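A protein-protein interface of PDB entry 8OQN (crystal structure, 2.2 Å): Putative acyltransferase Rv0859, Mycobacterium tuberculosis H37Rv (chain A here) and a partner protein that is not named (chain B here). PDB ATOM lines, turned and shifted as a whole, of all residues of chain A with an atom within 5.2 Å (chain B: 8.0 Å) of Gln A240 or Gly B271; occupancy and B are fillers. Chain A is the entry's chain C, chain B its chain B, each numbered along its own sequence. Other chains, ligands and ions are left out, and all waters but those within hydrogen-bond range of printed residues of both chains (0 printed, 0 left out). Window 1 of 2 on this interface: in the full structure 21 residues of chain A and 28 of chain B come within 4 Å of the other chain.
Hydrophobic or aromatic side chains of chain B that line the printed part of chain A: Leu B648. Of the 10 printed residues of chain A, 6 touch a printed residue of chain B. Printed residues of chain A that touch a printed residue of chain B: Met A145, Asp A236, Val A237, Leu A239, Gln A240 and His A243. Hydrophobic or aromatic side chains of chain A that line the printed part of chain B: Met A145, Val A237, Leu A239 and His A243.
Among the printed residues, pairs that only touch across the chains: Asp A236 with Lys B267 (3.2 Å), Gln A240 with Lys B270 (3.5 Å), His A243 with Leu B648 (3.6 Å), Val A237 with Ser B263 (3.7 Å), His A243 with Gln B553 (3.7 Å), Met A145 with Arg B266 (3.7 Å), Gln A240 with Gln B553 (3.8 Å) and Val A237 with Arg B266 (3.9 Å).
N of Gly B271 lies within hydrogen-bond range of O of Arg B266 (3.2 Å). The side-chain amide oxygen (OE1) of Gln B553 sits at hydrogen-bond distance from the side-chain amide nitrogen (NE2) of Gln B557 (2.9 Å).
Printed residues of chain A within 4 Å of Gly B271: Gln A240. Of the printed residues of chain B, Leu A239 touches Gln B553. Printed residues of chain A within 4 Å of Gln B553: Leu A239, Gln A240 and His A243. Ala B272 touches none of the printed residues of chain A. The nearest residue of chain B that does not touch Gln A240 is Leu B648 (4.2 Å). The nearest printed residue of chain A that does not touch Gly B271 is Met A145 (6.9 Å).
OE1 of Gln A240 is in hydrogen-bond range of NE of Arg B266 (3.1 Å). N of Gly B271 sits close to NE2 of Gln A240, 3.4 Å away. The side-chain amide nitrogen of Gln B553 is in hydrogen-bond range of the backbone carbonyl oxygen of Leu A239, at 3.4 Å. The backbone carbonyl oxygen (O) of Gln A240 is in hydrogen-bond range of the side-chain amide nitrogen (NE2) of Gln B557 (3.0 Å).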
ATOM      1  N   MET A 145       7.661 -11.699   5.953  1.00  0.00           N
ATOM      2  CA  MET A 145       8.983 -12.207   5.588  1.00  0.00           C
ATOM      3  C   MET A 145       9.698 -11.236   4.643  1.00  0.00           C
ATOM      4  O   MET A 145      10.001 -11.547   3.489  1.00  0.00           O
ATOM      5  CB  MET A 145       8.875 -13.612   4.983  1.00  0.00           C
ATOM      6  CG  MET A 145       8.050 -14.573   5.830  1.00  0.00           C
ATOM      7  SD  MET A 145       7.848 -16.208   5.093  1.00  0.00           S
ATOM      8  CE  MET A 145       9.460 -16.932   5.392  1.00  0.00           C
ATOM      9  N   ASP A 235      18.978 -14.044   3.881  1.00  0.00           N
ATOM     10  CA  ASP A 235      19.142 -15.263   3.092  1.00  0.00           C
ATOM     11  C   ASP A 235      18.292 -16.393   3.658  1.00  0.00           C
ATOM     12  O   ASP A 235      17.591 -17.092   2.918  1.00  0.00           O
ATOM     13  CB  ASP A 235      20.616 -15.671   3.050  1.00  0.00           C
ATOM     14  CG  ASP A 235      21.316 -15.211   1.785  1.00  0.00           C
ATOM     15  OD1 ASP A 235      21.085 -14.059   1.357  1.00  0.00           O
ATOM     16  OD2 ASP A 235      22.105 -16.003   1.226  1.00  0.00           O
ATOM     17  N   ASP A 236      18.331 -16.575   4.981  1.00  0.00           N
ATOM     18  CA  ASP A 236      17.566 -17.651   5.601  1.00  0.00           C
ATOM     19  C   ASP A 236      16.068 -17.395   5.506  1.00  0.00           C
ATOM     20  O   ASP A 236      15.288 -18.331   5.298  1.00  0.00           O
ATOM     21  CB  ASP A 236      17.994 -17.827   7.056  1.00  0.00           C
ATOM     22  CG  ASP A 236      19.392 -18.398   7.185  1.00  0.00           C
ATOM     23  OD1 ASP A 236      20.147 -18.358   6.190  1.00  0.00           O
ATOM     24  OD2 ASP A 236      19.732 -18.901   8.276  1.00  0.00           O
ATOM     25  N   VAL A 237      15.643 -16.138   5.661  1.00  0.00           N
ATOM     26  CA  VAL A 237      14.224 -15.813   5.521  1.00  0.00           C
ATOM     27  C   VAL A 237      13.745 -16.128   4.110  1.00  0.00           C
ATOM     28  O   VAL A 237      12.658 -16.687   3.917  1.00  0.00           O
ATOM     29  CB  VAL A 237      13.968 -14.341   5.891  1.00  0.00           C
ATOM     30  CG1 VAL A 237      12.516 -13.976   5.626  1.00  0.00           C
ATOM     31  CG2 VAL A 237      14.320 -14.086   7.343  1.00  0.00           C
ATOM     32  N   ALA A 238      14.552 -15.781   3.104  1.00  0.00           N
ATOM     33  CA  ALA A 238      14.183 -16.067   1.722  1.00  0.00           C
ATOM     34  C   ALA A 238      14.055 -17.566   1.481  1.00  0.00           C
ATOM     35  O   ALA A 238      13.114 -18.018   0.818  1.00  0.00           O
ATOM     36  CB  ALA A 238      15.211 -15.456   0.770  1.00  0.00           C
ATOM     37  N   LEU A 239      14.988 -18.353   2.018  1.00  0.00           N
ATOM     38  CA  LEU A 239      14.959 -19.794   1.806  1.00  0.00           C
ATOM     39  C   LEU A 239      13.917 -20.498   2.663  1.00  0.00           C
ATOM     40  O   LEU A 239      13.554 -21.638   2.354  1.00  0.00           O
ATOM     41  CB  LEU A 239      16.341 -20.394   2.069  1.00  0.00           C
ATOM     42  CG  LEU A 239      17.434 -19.894   1.122  1.00  0.00           C
ATOM     43  CD1 LEU A 239      18.718 -20.680   1.308  1.00  0.00           C
ATOM     44  CD2 LEU A 239      16.957 -19.959  -0.322  1.00  0.00           C
ATOM     45  N   GLN A 240      13.430 -19.858   3.728  1.00  0.00           N
ATOM     46  CA  GLN A 240      12.319 -20.438   4.475  1.00  0.00           C
ATOM     47  C   GLN A 240      11.049 -20.462   3.637  1.00  0.00           C
ATOM     48  O   GLN A 240      10.232 -21.379   3.776  1.00  0.00           O
ATOM     49  CB  GLN A 240      12.092 -19.672   5.779  1.00  0.00           C
ATOM     50  CG  GLN A 240      13.116 -19.988   6.859  1.00  0.00           C
ATOM     51  CD  GLN A 240      12.938 -19.150   8.111  1.00  0.00           C
ATOM     52  OE1 GLN A 240      11.875 -18.572   8.344  1.00  0.00           O
ATOM     53  NE2 GLN A 240      13.987 -19.073   8.923  1.00  0.00           N
ATOM     54  N   LYS A 241      10.867 -19.475   2.759  1.00  0.00           N
ATOM     55  CA  LYS A 241       9.738 -19.509   1.839  1.00  0.00           C
ATOM     56  C   LYS A 241      10.060 -20.302   0.577  1.00  0.00           C
ATOM     57  O   LYS A 241       9.252 -21.123   0.134  1.00  0.00           O
ATOM     58  CB  LYS A 241       9.296 -18.092   1.468  1.00  0.00           C
ATOM     59  CG  LYS A 241       8.112 -18.098   0.518  1.00  0.00           C
ATOM     60  CD  LYS A 241       7.519 -16.727   0.307  1.00  0.00           C
ATOM     61  CE  LYS A 241       6.187 -16.833  -0.419  1.00  0.00           C
ATOM     62  NZ  LYS A 241       5.033 -16.557   0.483  1.00  0.00           N
ATOM     63  N   TYR A 242      11.230 -20.070  -0.014  1.00  0.00           N
ATOM     64  CA  TYR A 242      11.649 -20.810  -1.205  1.00  0.00           C
ATOM     65  C   TYR A 242      12.467 -22.024  -0.762  1.00  0.00           C
ATOM     66  O   TYR A 242      13.674 -22.138  -0.988  1.00  0.00           O
ATOM     67  CB  TYR A 242      12.409 -19.897  -2.156  1.00  0.00           C
ATOM     68  CG  TYR A 242      11.496 -18.886  -2.816  1.00  0.00           C
ATOM     69  CD1 TYR A 242      11.162 -17.698  -2.177  1.00  0.00           C
ATOM     70  CD2 TYR A 242      10.940 -19.136  -4.063  1.00  0.00           C
ATOM     71  CE1 TYR A 242      10.314 -16.780  -2.769  1.00  0.00           C
ATOM     72  CE2 TYR A 242      10.091 -18.225  -4.664  1.00  0.00           C
ATOM     73  CZ  TYR A 242       9.781 -17.049  -4.013  1.00  0.00           C
ATOM     74  OH  TYR A 242       8.935 -16.146  -4.612  1.00  0.00           O
ATOM     75  N   HIS A 243      11.754 -22.952  -0.121  1.00  0.00           N
ATOM     76  CA  HIS A 243      12.393 -24.015   0.642  1.00  0.00           C
ATOM     77  C   HIS A 243      13.043 -25.074  -0.236  1.00  0.00           C
ATOM     78  O   HIS A 243      13.858 -25.854   0.266  1.00  0.00           O
ATOM     79  CB  HIS A 243      11.373 -24.663   1.580  1.00  0.00           C
ATOM     80  CG  HIS A 243      10.090 -25.039   0.910  1.00  0.00           C
ATOM     81  ND1 HIS A 243       9.989 -26.100   0.037  1.00  0.00           N
ATOM     82  CD2 HIS A 243       8.853 -24.496   0.987  1.00  0.00           C
ATOM     83  CE1 HIS A 243       8.744 -26.196  -0.393  1.00  0.00           C
ATOM     84  NE2 HIS A 243       8.034 -25.234   0.168  1.00  0.00           N
ATOM     85  N   PRO B 262      13.792  -8.667  12.929  1.00  0.00           N
ATOM     86  CA  PRO B 262      12.915  -9.837  12.740  1.00  0.00           C
ATOM     87  C   PRO B 262      13.548 -10.933  11.904  1.00  0.00           C
ATOM     88  O   PRO B 262      13.310 -12.118  12.169  1.00  0.00           O
ATOM     89  CB  PRO B 262      11.678  -9.241  12.051  1.00  0.00           C
ATOM     90  CG  PRO B 262      11.708  -7.794  12.400  1.00  0.00           C
ATOM     91  CD  PRO B 262      13.158  -7.438  12.419  1.00  0.00           C
ATOM     92  N   SER B 263      14.357 -10.576  10.902  1.00  0.00           N
ATOM     93  CA  SER B 263      14.956 -11.593  10.042  1.00  0.00           C
ATOM     94  C   SER B 263      16.018 -12.391  10.787  1.00  0.00           C
ATOM     95  O   SER B 263      16.136 -13.606  10.596  1.00  0.00           O
ATOM     96  CB  SER B 263      15.546 -10.944   8.792  1.00  0.00           C
ATOM     97  OG  SER B 263      16.580 -10.037   9.129  1.00  0.00           O
ATOM     98  N   ASN B 264      16.806 -11.725  11.635  1.00  0.00           N
ATOM     99  CA  ASN B 264      17.754 -12.454  12.472  1.00  0.00           C
ATOM    100  C   ASN B 264      17.027 -13.348  13.468  1.00  0.00           C
ATOM    101  O   ASN B 264      17.503 -14.440  13.792  1.00  0.00           O
ATOM    102  CB  ASN B 264      18.678 -11.478  13.197  1.00  0.00           C
ATOM    103  CG  ASN B 264      19.863 -11.057  12.350  1.00  0.00           C
ATOM    104  OD1 ASN B 264      20.596 -11.895  11.825  1.00  0.00           O
ATOM    105  ND2 ASN B 264      20.054  -9.749  12.206  1.00  0.00           N
ATOM    106  N   LEU B 265      15.869 -12.902  13.959  1.00  0.00           N
ATOM    107  CA  LEU B 265      15.079 -13.733  14.861  1.00  0.00           C
ATOM    108  C   LEU B 265      14.556 -14.969  14.139  1.00  0.00           C
ATOM    109  O   LEU B 265      14.612 -16.084  14.671  1.00  0.00           O
ATOM    110  CB  LEU B 265      13.927 -12.920  15.453  1.00  0.00           C
ATOM    111  CG  LEU B 265      13.076 -13.633  16.506  1.00  0.00           C
ATOM    112  CD1 LEU B 265      13.943 -14.112  17.665  1.00  0.00           C
ATOM    113  CD2 LEU B 265      11.959 -12.729  17.007  1.00  0.00           C
ATOM    114  N   ARG B 266      14.036 -14.787  12.920  1.00  0.00           N
ATOM    115  CA  ARG B 266      13.639 -15.932  12.107  1.00  0.00           C
ATOM    116  C   ARG B 266      14.818 -16.856  11.830  1.00  0.00           C
ATOM    117  O   ARG B 266      14.644 -18.078  11.740  1.00  0.00           O
ATOM    118  CB  ARG B 266      13.023 -15.466  10.785  1.00  0.00           C
ATOM    119  CG  ARG B 266      11.661 -14.800  10.900  1.00  0.00           C
ATOM    120  CD  ARG B 266      10.957 -14.770   9.546  1.00  0.00           C
ATOM    121  NE  ARG B 266      10.370 -16.062   9.207  1.00  0.00           N
ATOM    122  CZ  ARG B 266       9.072 -16.329   9.255  1.00  0.00           C
ATOM    123  NH1 ARG B 266       8.190 -15.403   9.596  1.00  0.00           N
ATOM    124  NH2 ARG B 266       8.647 -17.550   8.945  1.00  0.00           N
ATOM    125  N   LYS B 267      16.021 -16.293  11.691  1.00  0.00           N
ATOM    126  CA  LYS B 267      17.203 -17.110  11.437  1.00  0.00           C
ATOM    127  C   LYS B 267      17.539 -17.986  12.638  1.00  0.00           C
ATOM    128  O   LYS B 267      17.933 -19.147  12.476  1.00  0.00           O
ATOM    129  CB  LYS B 267      18.391 -16.215  11.084  1.00  0.00           C
ATOM    130  CG  LYS B 267      19.681 -16.966  10.815  1.00  0.00           C
ATOM    131  CD  LYS B 267      20.856 -16.012  10.695  1.00  0.00           C
ATOM    132  CE  LYS B 267      22.145 -16.768  10.419  1.00  0.00           C
ATOM    133  NZ  LYS B 267      23.333 -15.872  10.417  1.00  0.00           N
ATOM    134  N   GLN B 268      17.394 -17.445  13.851  1.00  0.00           N
ATOM    135  CA  GLN B 268      17.713 -18.216  15.048  1.00  0.00           C
ATOM    136  C   GLN B 268      16.668 -19.292  15.308  1.00  0.00           C
ATOM    137  O   GLN B 268      17.012 -20.430  15.647  1.00  0.00           O
ATOM    138  CB  GLN B 268      17.837 -17.285  16.255  1.00  0.00           C
ATOM    139  CG  GLN B 268      19.046 -16.367  16.199  1.00  0.00           C
ATOM    140  CD  GLN B 268      20.358 -17.130  16.243  1.00  0.00           C
ATOM    141  OE1 GLN B 268      20.643 -17.842  17.206  1.00  0.00           O
ATOM    142  NE2 GLN B 268      21.160 -16.989  15.192  1.00  0.00           N
ATOM    143  N   LEU B 269      15.387 -18.955  15.154  1.00  0.00           N
ATOM    144  CA  LEU B 269      14.319 -19.924  15.356  1.00  0.00           C
ATOM    145  C   LEU B 269      14.116 -20.838  14.155  1.00  0.00           C
ATOM    146  O   LEU B 269      13.318 -21.778  14.245  1.00  0.00           O
ATOM    147  CB  LEU B 269      13.009 -19.200  15.679  1.00  0.00           C
ATOM    148  CG  LEU B 269      13.035 -18.201  16.838  1.00  0.00           C
ATOM    149  CD1 LEU B 269      11.668 -17.565  17.032  1.00  0.00           C
ATOM    150  CD2 LEU B 269      13.502 -18.871  18.121  1.00  0.00           C
ATOM    151  N   LYS B 270      14.806 -20.578  13.041  1.00  0.00           N
ATOM    152  CA  LYS B 270      14.727 -21.408  11.839  1.00  0.00           C
ATOM    153  C   LYS B 270      13.299 -21.506  11.308  1.00  0.00           C
ATOM    154  O   LYS B 270      12.929 -22.491  10.666  1.00  0.00           O
ATOM    155  CB  LYS B 270      15.311 -22.801  12.092  1.00  0.00           C
ATOM    156  CG  LYS B 270      16.829 -22.817  12.207  1.00  0.00           C
ATOM    157  CD  LYS B 270      17.339 -24.086  12.868  1.00  0.00           C
ATOM    158  CE  LYS B 270      17.097 -24.060  14.368  1.00  0.00           C
ATOM    159  NZ  LYS B 270      17.726 -25.227  15.054  1.00  0.00           N
ATOM    160  N   GLY B 271      12.490 -20.482  11.571  1.00  0.00           N
ATOM    161  CA  GLY B 271      11.115 -20.462  11.116  1.00  0.00           C
ATOM    162  C   GLY B 271      10.148 -21.269  11.951  1.00  0.00           C
ATOM    163  O   GLY B 271       8.995 -21.439  11.536  1.00  0.00           O
ATOM    164  N   ALA B 272      10.576 -21.766  13.110  1.00  0.00           N
ATOM    165  CA  ALA B 272       9.697 -22.545  13.967  1.00  0.00           C
ATOM    166  C   ALA B 272       8.550 -21.676  14.484  1.00  0.00           C
ATOM    167  O   ALA B 272       8.696 -20.458  14.625  1.00  0.00           O
ATOM    168  CB  ALA B 272      10.479 -23.132  15.139  1.00  0.00           C
ATOM    169  N   PRO B 273       7.389 -22.280  14.768  1.00  0.00           N
ATOM    170  CA  PRO B 273       6.201 -21.500  15.156  1.00  0.00           C
ATOM    171  C   PRO B 273       6.108 -21.243  16.659  1.00  0.00           C
ATOM    172  O   PRO B 273       5.132 -21.614  17.319  1.00  0.00           O
ATOM    173  CB  PRO B 273       5.057 -22.385  14.651  1.00  0.00           C
ATOM    174  CG  PRO B 273       5.573 -23.773  14.826  1.00  0.00           C
ATOM    175  CD  PRO B 273       7.068 -23.706  14.575  1.00  0.00           C
ATOM    176  N   MET B 274       7.129 -20.589  17.213  1.00  0.00           N
ATOM    177  CA  MET B 274       7.074 -20.137  18.596  1.00  0.00           C
ATOM    178  C   MET B 274       6.662 -18.674  18.617  1.00  0.00           C
ATOM    179  O   MET B 274       7.430 -17.820  18.147  1.00  0.00           O
ATOM    180  CB  MET B 274       8.426 -20.323  19.287  1.00  0.00           C
ATOM    181  CG  MET B 274       8.813 -21.773  19.543  1.00  0.00           C
ATOM    182  SD  MET B 274       9.723 -21.982  21.089  1.00  0.00           S
ATOM    183  CE  MET B 274      11.067 -20.822  20.856  1.00  0.00           C
ATOM    184  N   GLN B 553      14.250 -28.175   5.274  1.00  0.00           N
ATOM    185  CA  GLN B 553      13.529 -26.977   5.689  1.00  0.00           C
ATOM    186  C   GLN B 553      12.303 -27.331   6.517  1.00  0.00           C
ATOM    187  O   GLN B 553      11.997 -26.657   7.508  1.00  0.00           O
ATOM    188  CB  GLN B 553      13.127 -26.150   4.467  1.00  0.00           C
ATOM    189  CG  GLN B 553      14.209 -25.211   3.961  1.00  0.00           C
ATOM    190  CD  GLN B 553      14.414 -24.011   4.868  1.00  0.00           C
ATOM    191  OE1 GLN B 553      13.629 -23.765   5.786  1.00  0.00           O
ATOM    192  NE2 GLN B 553      15.476 -23.257   4.616  1.00  0.00           N
ATOM    193  N   ALA B 554      11.589 -28.390   6.128  1.00  0.00           N
ATOM    194  CA  ALA B 554      10.417 -28.809   6.887  1.00  0.00           C
ATOM    195  C   ALA B 554      10.803 -29.277   8.284  1.00  0.00           C
ATOM    196  O   ALA B 554      10.078 -29.020   9.250  1.00  0.00           O
ATOM    197  CB  ALA B 554       9.671 -29.909   6.135  1.00  0.00           C
ATOM    198  N   SER B 556      13.454 -28.242  10.108  1.00  0.00           N
ATOM    199  CA  SER B 556      13.824 -27.079  10.909  1.00  0.00           C
ATOM    200  C   SER B 556      12.609 -26.222  11.238  1.00  0.00           C
ATOM    201  O   SER B 556      12.440 -25.789  12.384  1.00  0.00           O
ATOM    202  CB  SER B 556      14.880 -26.253  10.175  1.00  0.00           C
ATOM    203  OG  SER B 556      15.999 -27.051   9.837  1.00  0.00           O
ATOM    204  N   GLN B 557      11.746 -25.971  10.250  1.00  0.00           N
ATOM    205  CA  GLN B 557      10.565 -25.153  10.492  1.00  0.00           C
ATOM    206  C   GLN B 557       9.537 -25.864  11.362  1.00  0.00           C
ATOM    207  O   GLN B 557       8.699 -25.196  11.976  1.00  0.00           O
ATOM    208  CB  GLN B 557       9.934 -24.727   9.166  1.00  0.00           C
ATOM    209  CG  GLN B 557      10.810 -23.787   8.349  1.00  0.00           C
ATOM    210  CD  GLN B 557      10.115 -23.267   7.108  1.00  0.00           C
ATOM    211  OE1 GLN B 557       8.955 -22.858   7.156  1.00  0.00           O
ATOM    212  NE2 GLN B 557      10.823 -23.287   5.984  1.00  0.00           N
ATOM    213  N   ALA B 558       9.574 -27.197  11.425  1.00  0.00           N
ATOM    214  CA  ALA B 558       8.748 -27.909  12.390  1.00  0.00           C
ATOM    215  C   ALA B 558       9.225 -27.685  13.817  1.00  0.00           C
ATOM    216  O   ALA B 558       8.438 -27.852  14.757  1.00  0.00           O
ATOM    217  CB  ALA B 558       8.733 -29.405  12.079  1.00  0.00           C
ATOM    218  N   GLY B 559      10.488 -27.312  14.000  1.00  0.00           N
ATOM    219  CA  GLY B 559      11.038 -27.054  15.311  1.00  0.00           C
ATOM    220  C   GLY B 559      12.028 -28.078  15.821  1.00  0.00           C
ATOM    221  O   GLY B 559      12.435 -27.988  16.985  1.00  0.00           O
ATOM    222  N   LEU B 648       4.693 -27.352   1.983  1.00  0.00           N
ATOM    223  CA  LEU B 648       5.635 -27.469   3.092  1.00  0.00           C
ATOM    224  C   LEU B 648       4.928 -27.875   4.378  1.00  0.00           C
ATOM    225  O   LEU B 648       5.458 -28.672   5.161  1.00  0.00           O
ATOM    226  CB  LEU B 648       6.383 -26.150   3.288  1.00  0.00           C
ATOM    227  CG  LEU B 648       7.473 -26.158   4.361  1.00  0.00           C
ATOM    228  CD1 LEU B 648       8.653 -27.011   3.923  1.00  0.00           C
ATOM    229  CD2 LEU B 648       7.921 -24.743   4.689  1.00  0.00           C
ATOM    230  N   ILE B 652       5.767 -30.855   7.036  1.00  0.00           N
ATOM    231  CA  ILE B 652       5.925 -30.591   8.464  1.00  0.00           C
ATOM    232  C   ILE B 652       4.995 -31.485   9.274  1.00  0.00           C
ATOM    233  O   ILE B 652       5.419 -32.156  10.223  1.00  0.00           O
ATOM    234  CB  ILE B 652       5.679 -29.102   8.762  1.00  0.00           C
ATOM    235  CG1 ILE B 652       6.790 -28.248   8.150  1.00  0.00           C
ATOM    236  CG2 ILE B 652       5.563 -28.864  10.262  1.00  0.00           C
ATOM    237  CD1 ILE B 652       6.536 -26.755   8.241  1.00  0.00           C
ATOM    238  N   TRP B 691       7.821 -26.425  21.560  1.00  0.00           N
ATOM    239  CA  TRP B 691       6.584 -25.660  21.426  1.00  0.00           C
ATOM    240  C   TRP B 691       5.353 -26.555  21.434  1.00  0.00           C
ATOM    241  O   TRP B 691       4.252 -26.074  21.723  1.00  0.00           O
ATOM    242  CB  TRP B 691       6.606 -24.815  20.149  1.00  0.00           C
ATOM    243  CG  TRP B 691       6.560 -25.596  18.866  1.00  0.00           C
ATOM    244  CD1 TRP B 691       7.627 -26.008  18.119  1.00  0.00           C
ATOM    245  CD2 TRP B 691       5.388 -26.037  18.163  1.00  0.00           C
ATOM    246  NE1 TRP B 691       7.194 -26.684  17.005  1.00  0.00           N
ATOM    247  CE2 TRP B 691       5.824 -26.717  17.009  1.00  0.00           C
ATOM    248  CE3 TRP B 691       4.014 -25.932  18.404  1.00  0.00           C
ATOM    249  CZ2 TRP B 691       4.938 -27.289  16.097  1.00  0.00           C
ATOM    250  CZ3 TRP B 691       3.133 -26.497  17.494  1.00  0.00           C
ATOM    251  CH2 TRP B 691       3.600 -27.167  16.355  1.00  0.00           C
